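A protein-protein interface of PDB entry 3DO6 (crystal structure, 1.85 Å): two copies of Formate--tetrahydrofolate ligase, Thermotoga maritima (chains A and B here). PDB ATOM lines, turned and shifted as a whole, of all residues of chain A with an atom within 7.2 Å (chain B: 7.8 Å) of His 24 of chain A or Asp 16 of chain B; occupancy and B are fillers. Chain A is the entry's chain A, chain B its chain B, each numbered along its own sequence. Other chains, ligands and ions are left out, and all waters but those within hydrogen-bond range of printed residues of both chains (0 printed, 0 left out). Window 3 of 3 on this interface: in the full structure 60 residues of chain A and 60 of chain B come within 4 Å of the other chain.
Among the printed residues, pairs that only touch across the chains: Tyr 22 of chain A with Pro 21 of chain B (3.4 Å) and His 24 of chain A with Tyr 20 of chain B (3.7 Å).
Printed residues of chain A that touch a printed residue of chain B: Pro 21, Tyr 22, Gly 23 and His 24.
Of the 14 printed residues of chain B, 4 touch a printed residue of chain A.
Printed residues of chain B that touch a printed residue of chain A: Asp 16, Leu 19, Tyr 20 and Pro 21.
Hydrophobic or aromatic side chains of chain B within 4 Å of the printed part of chain A: Tyr 20 and Pro 21.
Among the printed residues, no Asp or Glu carboxylate lies within 4 Å of a Lys or Arg side-chain nitrogen of the other chain.
NE2 of His 24 of chain A sits close to O of Asp 16 of chain B (3.2 Å).
O of Pro 21 of chain B lies within hydrogen-bond range of N of Gly 23 of chain A (2.7 Å).
The backbone carbonyl oxygen (O) of Pro 21 of chain A sits close to the backbone carbonyl oxygen (O) of Pro 21 of chain B (3.2 Å).
The backbone carbonyl oxygen (O) of Leu 19 of chain B lies within hydrogen-bond range of a ring nitrogen (NE2) of His 24 of chain A (2.7 Å).
Asp 16 of chain B touches just one residue of chain A: His 24 (3.2 Å).
Of chain B, only Pro 21 comes within 4 Å of Gly 23 of chain A.
Printed residues of chain B within 4 Å of Pro 21 of chain A: Pro 21.
Of the printed residues of chain A, Pro 21 of chain B touches Pro 21 (3.2 Å), Tyr 22 (3.4 Å) and Gly 23 (2.7 Å).
Of the printed residues of chain A, Tyr 20 of chain B touches His 24.
The nearest residue of chain B that does not touch His 24 of chain A is Pro 21 of chain B (4.04 Å).
The backbone carbonyl oxygen (O) of Tyr 20 of chain B lies within hydrogen-bond range of the backbone NH (N) of Lys 28 of chain B (2.8 Å).
N of Ile 5 of chain A lies within hydrogen-bond range of O of His 24 of chain A, 2.8 Å away.
Pro 21 of chain A touches its own counterpart, Pro 21 of chain B.
Of the 6 pairs that touch across the chains among the printed residues, 1 has its exchanged pair printed and touching as well.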
ATOM      1  N   LYS A   3     -18.721 -22.579  13.924  1.00  0.00           N
ATOM      2  CA  LYS A   3     -17.520 -23.308  14.243  1.00  0.00           C
ATOM      3  C   LYS A   3     -17.274 -24.455  13.258  1.00  0.00           C
ATOM      4  O   LYS A   3     -18.179 -25.221  12.942  1.00  0.00           O
ATOM      5  CB  LYS A   3     -17.580 -23.856  15.657  1.00  0.00           C
ATOM      6  CG  LYS A   3     -17.923 -22.812  16.717  1.00  0.00           C
ATOM      7  CD  LYS A   3     -17.814 -23.445  18.090  1.00  0.00           C
ATOM      8  CE  LYS A   3     -17.674 -22.407  19.218  1.00  0.00           C
ATOM      9  NZ  LYS A   3     -17.788 -23.078  20.562  1.00  0.00           N
ATOM     10  N   PRO A   4     -16.030 -24.582  12.780  1.00  0.00           N
ATOM     11  CA  PRO A   4     -15.645 -25.808  12.086  1.00  0.00           C
ATOM     12  C   PRO A   4     -15.937 -27.023  12.925  1.00  0.00           C
ATOM     13  O   PRO A   4     -15.793 -27.024  14.153  1.00  0.00           O
ATOM     14  CB  PRO A   4     -14.124 -25.659  11.911  1.00  0.00           C
ATOM     15  CG  PRO A   4     -13.849 -24.217  12.067  1.00  0.00           C
ATOM     16  CD  PRO A   4     -14.857 -23.732  13.063  1.00  0.00           C
ATOM     17  N   ILE A   5     -16.353 -28.074  12.253  1.00  0.00           N
ATOM     18  CA  ILE A   5     -16.840 -29.251  12.978  1.00  0.00           C
ATOM     19  C   ILE A   5     -15.732 -29.843  13.869  1.00  0.00           C
ATOM     20  O   ILE A   5     -16.008 -30.433  14.902  1.00  0.00           O
ATOM     21  CB  ILE A   5     -17.472 -30.311  12.003  1.00  0.00           C
ATOM     22  CG1 ILE A   5     -18.403 -31.232  12.793  1.00  0.00           C
ATOM     23  CG2 ILE A   5     -16.407 -31.051  11.175  1.00  0.00           C
ATOM     24  CD1 ILE A   5     -19.520 -30.512  13.461  1.00  0.00           C
ATOM     25  N   LYS A   6     -14.479 -29.681  13.477  1.00  0.00           N
ATOM     26  CA  LYS A   6     -13.381 -30.253  14.280  1.00  0.00           C
ATOM     27  C   LYS A   6     -13.399 -29.613  15.666  1.00  0.00           C
ATOM     28  O   LYS A   6     -13.013 -30.219  16.662  1.00  0.00           O
ATOM     29  CB  LYS A   6     -12.006 -30.063  13.626  1.00  0.00           C
ATOM     30  CG  LYS A   6     -11.282 -28.790  14.045  1.00  0.00           C
ATOM     31  N   GLU A   7     -13.883 -28.381  15.717  1.00  0.00           N
ATOM     32  CA  GLU A   7     -13.929 -27.644  16.978  1.00  0.00           C
ATOM     33  C   GLU A   7     -14.937 -28.323  17.874  1.00  0.00           C
ATOM     34  O   GLU A   7     -14.661 -28.619  19.042  1.00  0.00           O
ATOM     35  CB  GLU A   7     -14.333 -26.180  16.778  1.00  0.00           C
ATOM     36  CG  GLU A   7     -14.406 -25.405  18.100  1.00  0.00           C
ATOM     37  CD  GLU A   7     -14.154 -23.913  17.942  1.00  0.00           C
ATOM     38  OE1 GLU A   7     -13.552 -23.530  16.923  1.00  0.00           O
ATOM     39  OE2 GLU A   7     -14.562 -23.128  18.827  1.00  0.00           O
ATOM     40  N   PRO A  21     -15.802 -36.465   7.930  1.00  0.00           N
ATOM     41  CA  PRO A  21     -16.386 -35.183   7.571  1.00  0.00           C
ATOM     42  C   PRO A  21     -17.257 -35.175   6.326  1.00  0.00           C
ATOM     43  O   PRO A  21     -17.090 -35.978   5.407  1.00  0.00           O
ATOM     44  CB  PRO A  21     -15.158 -34.264   7.398  1.00  0.00           C
ATOM     45  CG  PRO A  21     -14.040 -35.177   7.132  1.00  0.00           C
ATOM     46  CD  PRO A  21     -14.333 -36.422   7.889  1.00  0.00           C
ATOM     47  N   TYR A  22     -18.234 -34.285   6.383  1.00  0.00           N
ATOM     48  CA  TYR A  22     -19.035 -33.896   5.239  1.00  0.00           C
ATOM     49  C   TYR A  22     -18.922 -32.391   5.101  1.00  0.00           C
ATOM     50  O   TYR A  22     -19.670 -31.605   5.719  1.00  0.00           O
ATOM     51  CB  TYR A  22     -20.494 -34.356   5.394  1.00  0.00           C
ATOM     52  CG  TYR A  22     -20.699 -35.861   5.265  1.00  0.00           C
ATOM     53  CD1 TYR A  22     -20.354 -36.745   6.295  1.00  0.00           C
ATOM     54  CD2 TYR A  22     -21.259 -36.400   4.106  1.00  0.00           C
ATOM     55  CE1 TYR A  22     -20.545 -38.120   6.147  1.00  0.00           C
ATOM     56  CE2 TYR A  22     -21.467 -37.769   3.975  1.00  0.00           C
ATOM     57  CZ  TYR A  22     -21.137 -38.621   4.964  1.00  0.00           C
ATOM     58  OH  TYR A  22     -21.370 -39.985   4.765  1.00  0.00           O
ATOM     59  N   GLY A  23     -17.946 -31.968   4.300  1.00  0.00           N
ATOM     60  CA  GLY A  23     -17.586 -30.561   4.274  1.00  0.00           C
ATOM     61  C   GLY A  23     -16.897 -30.191   5.561  1.00  0.00           C
ATOM     62  O   GLY A  23     -16.333 -31.030   6.228  1.00  0.00           O
ATOM     63  N   HIS A  24     -16.981 -28.920   5.904  1.00  0.00           N
ATOM     64  CA  HIS A  24     -16.233 -28.343   7.033  1.00  0.00           C
ATOM     65  C   HIS A  24     -17.044 -28.239   8.339  1.00  0.00           C
ATOM     66  O   HIS A  24     -16.479 -28.077   9.407  1.00  0.00           O
ATOM     67  CB  HIS A  24     -15.735 -26.956   6.618  1.00  0.00           C
ATOM     68  CG  HIS A  24     -14.787 -26.996   5.453  1.00  0.00           C
ATOM     69  ND1 HIS A  24     -14.911 -26.167   4.355  1.00  0.00           N
ATOM     70  CD2 HIS A  24     -13.720 -27.795   5.208  1.00  0.00           C
ATOM     71  CE1 HIS A  24     -13.945 -26.438   3.495  1.00  0.00           C
ATOM     72  NE2 HIS A  24     -13.211 -27.422   3.988  1.00  0.00           N
ATOM     73  N   TYR A  25     -18.361 -28.400   8.226  1.00  0.00           N
ATOM     74  CA  TYR A  25     -19.286 -28.129   9.340  1.00  0.00           C
ATOM     75  C   TYR A  25     -20.178 -29.305   9.777  1.00  0.00           C
ATOM     76  O   TYR A  25     -21.030 -29.165  10.628  1.00  0.00           O
ATOM     77  CB  TYR A  25     -20.139 -26.940   8.944  1.00  0.00           C
ATOM     78  CG  TYR A  25     -19.263 -25.751   8.655  1.00  0.00           C
ATOM     79  CD1 TYR A  25     -18.561 -25.146   9.675  1.00  0.00           C
ATOM     80  CD2 TYR A  25     -19.101 -25.261   7.359  1.00  0.00           C
ATOM     81  CE1 TYR A  25     -17.747 -24.060   9.439  1.00  0.00           C
ATOM     82  CE2 TYR A  25     -18.287 -24.183   7.114  1.00  0.00           C
ATOM     83  CZ  TYR A  25     -17.611 -23.585   8.161  1.00  0.00           C
ATOM     84  OH  TYR A  25     -16.783 -22.508   7.922  1.00  0.00           O
ATOM     85  N   ILE A  26     -19.946 -30.461   9.187  1.00  0.00           N
ATOM     86  CA  ILE A  26     -20.690 -31.678   9.540  1.00  0.00           C
ATOM     87  C   ILE A  26     -19.760 -32.861   9.549  1.00  0.00           C
ATOM     88  O   ILE A  26     -18.820 -32.918   8.745  1.00  0.00           O
ATOM     89  CB  ILE A  26     -21.835 -31.964   8.508  1.00  0.00           C
ATOM     90  CG1 ILE A  26     -22.734 -30.763   8.300  1.00  0.00           C
ATOM     91  CG2 ILE A  26     -22.609 -33.252   8.882  1.00  0.00           C
ATOM     92  CD1 ILE A  26     -23.544 -30.837   6.982  1.00  0.00           C
ATOM     93  N   ALA A  27     -19.997 -33.799  10.466  1.00  0.00           N
ATOM     94  CA  ALA A  27     -19.344 -35.115  10.419  1.00  0.00           C
ATOM     95  C   ALA A  27     -20.190 -36.259  10.938  1.00  0.00           C
ATOM     96  O   ALA A  27     -21.026 -36.092  11.809  1.00  0.00           O
ATOM     97  CB  ALA A  27     -18.023 -35.097  11.198  1.00  0.00           C
ATOM     98  N   GLN A 247     -24.013 -28.617  15.165  1.00  0.00           N
ATOM     99  CA  GLN A 247     -23.941 -27.651  16.266  1.00  0.00           C
ATOM    100  C   GLN A 247     -25.170 -26.796  16.321  1.00  0.00           C
ATOM    101  O   GLN A 247     -25.913 -26.687  15.363  1.00  0.00           O
ATOM    102  CB  GLN A 247     -22.689 -26.747  16.117  1.00  0.00           C
ATOM    103  CG  GLN A 247     -22.804 -25.631  15.072  1.00  0.00           C
ATOM    104  CD  GLN A 247     -21.446 -25.052  14.696  1.00  0.00           C
ATOM    105  OE1 GLN A 247     -21.001 -24.035  15.248  1.00  0.00           O
ATOM    106  NE2 GLN A 247     -20.786 -25.694  13.747  1.00  0.00           N
ATOM    107  N   ILE B   5      -7.038 -37.989   1.251  1.00  0.00           N
ATOM    108  CA  ILE B   5      -7.377 -37.098   0.175  1.00  0.00           C
ATOM    109  C   ILE B   5      -6.507 -35.845   0.188  1.00  0.00           C
ATOM    110  O   ILE B   5      -6.282 -35.205  -0.845  1.00  0.00           O
ATOM    111  CB  ILE B   5      -8.872 -36.719   0.194  1.00  0.00           C
ATOM    112  CG1 ILE B   5      -9.213 -36.142  -1.158  1.00  0.00           C
ATOM    113  CG2 ILE B   5      -9.188 -35.813   1.379  1.00  0.00           C
ATOM    114  CD1 ILE B   5      -8.922 -37.110  -2.282  1.00  0.00           C
ATOM    115  N   LYS B   6      -6.021 -35.493   1.368  1.00  0.00           N
ATOM    116  CA  LYS B   6      -5.237 -34.255   1.514  1.00  0.00           C
ATOM    117  C   LYS B   6      -3.964 -34.396   0.676  1.00  0.00           C
ATOM    118  O   LYS B   6      -3.454 -33.443   0.088  1.00  0.00           O
ATOM    119  CB  LYS B   6      -4.908 -33.985   2.993  1.00  0.00           C
ATOM    120  N   ALA B   9      -4.795 -33.893  -2.901  1.00  0.00           N
ATOM    121  CA  ALA B   9      -5.171 -32.522  -3.132  1.00  0.00           C
ATOM    122  C   ALA B   9      -3.922 -31.674  -3.150  1.00  0.00           C
ATOM    123  O   ALA B   9      -3.822 -30.690  -3.874  1.00  0.00           O
ATOM    124  CB  ALA B   9      -6.125 -32.039  -2.048  1.00  0.00           C
ATOM    125  N   ASP B  10      -2.958 -32.091  -2.345  1.00  0.00           N
ATOM    126  CA  ASP B  10      -1.647 -31.392  -2.277  1.00  0.00           C
ATOM    127  C   ASP B  10      -0.890 -31.517  -3.598  1.00  0.00           C
ATOM    128  O   ASP B  10      -0.258 -30.576  -4.065  1.00  0.00           O
ATOM    129  CB  ASP B  10      -0.782 -31.939  -1.145  1.00  0.00           C
ATOM    130  CG  ASP B  10      -1.159 -31.357   0.203  1.00  0.00           C
ATOM    131  OD1 ASP B  10      -1.853 -30.313   0.214  1.00  0.00           O
ATOM    132  OD2 ASP B  10      -0.782 -31.962   1.242  1.00  0.00           O
ATOM    133  N   GLU B  13      -2.036 -28.971  -5.563  1.00  0.00           N
ATOM    134  CA  GLU B  13      -1.867 -27.701  -4.890  1.00  0.00           C
ATOM    135  C   GLU B  13      -3.176 -27.008  -4.535  1.00  0.00           C
ATOM    136  O   GLU B  13      -3.285 -25.774  -4.547  1.00  0.00           O
ATOM    137  CB  GLU B  13      -0.991 -26.789  -5.751  1.00  0.00           C
ATOM    138  CG  GLU B  13       0.403 -27.406  -5.946  1.00  0.00           C
ATOM    139  CD  GLU B  13       1.373 -26.528  -6.715  1.00  0.00           C
ATOM    140  OE1 GLU B  13       1.287 -25.283  -6.617  1.00  0.00           O
ATOM    141  OE2 GLU B  13       2.239 -27.104  -7.405  1.00  0.00           O
ATOM    142  N   LEU B  14      -4.168 -27.830  -4.220  1.00  0.00           N
ATOM    143  CA  LEU B  14      -5.493 -27.336  -3.802  1.00  0.00           C
ATOM    144  C   LEU B  14      -5.523 -26.990  -2.326  1.00  0.00           C
ATOM    145  O   LEU B  14      -5.023 -27.738  -1.492  1.00  0.00           O
ATOM    146  CB  LEU B  14      -6.573 -28.376  -4.108  1.00  0.00           C
ATOM    147  CG  LEU B  14      -6.623 -28.788  -5.577  1.00  0.00           C
ATOM    148  CD1 LEU B  14      -7.596 -29.946  -5.786  1.00  0.00           C
ATOM    149  CD2 LEU B  14      -6.914 -27.554  -6.435  1.00  0.00           C
ATOM    150  N   LYS B  15      -6.135 -25.846  -2.033  1.00  0.00           N
ATOM    151  CA  LYS B  15      -6.292 -25.348  -0.658  1.00  0.00           C
ATOM    152  C   LYS B  15      -7.641 -25.710  -0.026  1.00  0.00           C
ATOM    153  O   LYS B  15      -8.654 -25.876  -0.704  1.00  0.00           O
ATOM    154  CB  LYS B  15      -6.065 -23.830  -0.621  1.00  0.00           C
ATOM    155  CG  LYS B  15      -4.621 -23.395  -0.929  1.00  0.00           C
ATOM    156  N   ASP B  16      -7.613 -25.867   1.292  1.00  0.00           N
ATOM    157  CA  ASP B  16      -8.803 -26.295   2.075  1.00  0.00           C
ATOM    158  C   ASP B  16     -10.024 -25.462   1.824  1.00  0.00           C
ATOM    159  O   ASP B  16     -11.147 -25.903   2.044  1.00  0.00           O
ATOM    160  CB  ASP B  16      -8.540 -26.234   3.581  1.00  0.00           C
ATOM    161  CG  ASP B  16      -7.776 -27.406   4.068  1.00  0.00           C
ATOM    162  OD1 ASP B  16      -7.930 -28.486   3.464  1.00  0.00           O
ATOM    163  OD2 ASP B  16      -7.018 -27.239   5.050  1.00  0.00           O
ATOM    164  N   ASP B  17      -9.789 -24.243   1.389  1.00  0.00           N
ATOM    165  CA  ASP B  17     -10.863 -23.265   1.273  1.00  0.00           C
ATOM    166  C   ASP B  17     -11.766 -23.534   0.065  1.00  0.00           C
ATOM    167  O   ASP B  17     -12.825 -22.943  -0.074  1.00  0.00           O
ATOM    168  CB  ASP B  17     -10.330 -21.830   1.247  1.00  0.00           C
ATOM    169  CG  ASP B  17      -9.432 -21.558   0.071  1.00  0.00           C
ATOM    170  OD1 ASP B  17      -8.788 -22.499  -0.422  1.00  0.00           O
ATOM    171  OD2 ASP B  17      -9.355 -20.390  -0.350  1.00  0.00           O
ATOM    172  N   ILE B  18     -11.336 -24.459  -0.787  1.00  0.00           N
ATOM    173  CA  ILE B  18     -12.155 -24.873  -1.945  1.00  0.00           C
ATOM    174  C   ILE B  18     -12.344 -26.382  -1.991  1.00  0.00           C
ATOM    175  O   ILE B  18     -12.801 -26.949  -2.995  1.00  0.00           O
ATOM    176  CB  ILE B  18     -11.615 -24.325  -3.307  1.00  0.00           C
ATOM    177  CG1 ILE B  18     -10.138 -24.654  -3.541  1.00  0.00           C
ATOM    178  CG2 ILE B  18     -11.811 -22.816  -3.372  1.00  0.00           C
ATOM    179  CD1 ILE B  18      -9.841 -26.085  -3.948  1.00  0.00           C
ATOM    180  N   LEU B  19     -11.983 -27.010  -0.880  1.00  0.00           N
ATOM    181  CA  LEU B  19     -12.089 -28.437  -0.717  1.00  0.00           C
ATOM    182  C   LEU B  19     -13.078 -28.803   0.355  1.00  0.00           C
ATOM    183  O   LEU B  19     -13.026 -28.305   1.484  1.00  0.00           O
ATOM    184  CB  LEU B  19     -10.767 -29.039  -0.323  1.00  0.00           C
ATOM    185  CG  LEU B  19      -9.676 -29.200  -1.359  1.00  0.00           C
ATOM    186  CD1 LEU B  19      -8.519 -29.935  -0.662  1.00  0.00           C
ATOM    187  CD2 LEU B  19     -10.171 -29.979  -2.617  1.00  0.00           C
ATOM    188  N   TYR B  20     -13.981 -29.706  -0.015  1.00  0.00           N
ATOM    189  CA  TYR B  20     -15.016 -30.182   0.898  1.00  0.00           C
ATOM    190  C   TYR B  20     -14.853 -31.678   1.047  1.00  0.00           C
ATOM    191  O   TYR B  20     -15.182 -32.443   0.132  1.00  0.00           O
ATOM    192  CB  TYR B  20     -16.395 -29.840   0.365  1.00  0.00           C
ATOM    193  CG  TYR B  20     -16.490 -28.407  -0.027  1.00  0.00           C
ATOM    194  CD1 TYR B  20     -16.392 -27.404   0.924  1.00  0.00           C
ATOM    195  CD2 TYR B  20     -16.669 -28.038  -1.355  1.00  0.00           C
ATOM    196  CE1 TYR B  20     -16.461 -26.080   0.569  1.00  0.00           C
ATOM    197  CE2 TYR B  20     -16.740 -26.726  -1.718  1.00  0.00           C
ATOM    198  CZ  TYR B  20     -16.623 -25.744  -0.750  1.00  0.00           C
ATOM    199  OH  TYR B  20     -16.702 -24.420  -1.112  1.00  0.00           O
ATOM    200  N   PRO B  21     -14.313 -32.118   2.182  1.00  0.00           N
ATOM    201  CA  PRO B  21     -14.141 -33.545   2.296  1.00  0.00           C
ATOM    202  C   PRO B  21     -15.401 -34.337   2.511  1.00  0.00           C
ATOM    203  O   PRO B  21     -16.377 -33.872   3.096  1.00  0.00           O
ATOM    204  CB  PRO B  21     -13.190 -33.693   3.488  1.00  0.00           C
ATOM    205  CG  PRO B  21     -13.431 -32.491   4.313  1.00  0.00           C
ATOM    206  CD  PRO B  21     -13.849 -31.396   3.375  1.00  0.00           C
ATOM    207  N   LYS B  28     -15.001 -32.899  -2.661  1.00  0.00           N
ATOM    208  CA  LYS B  28     -15.501 -32.012  -3.713  1.00  0.00           C
ATOM    209  C   LYS B  28     -14.569 -30.812  -3.812  1.00  0.00           C
ATOM    210  O   LYS B  28     -13.999 -30.375  -2.809  1.00  0.00           O
ATOM    211  CB  LYS B  28     -16.937 -31.548  -3.453  1.00  0.00           C
ATOM    212  CG  LYS B  28     -17.969 -32.606  -3.821  1.00  0.00           C
ATOM    213  CD  LYS B  28     -19.410 -32.088  -3.761  1.00  0.00           C
ATOM    214  CE  LYS B  28     -20.380 -33.159  -4.246  1.00  0.00           C
ATOM    215  NZ  LYS B  28     -20.278 -33.468  -5.718  1.00  0.00           N
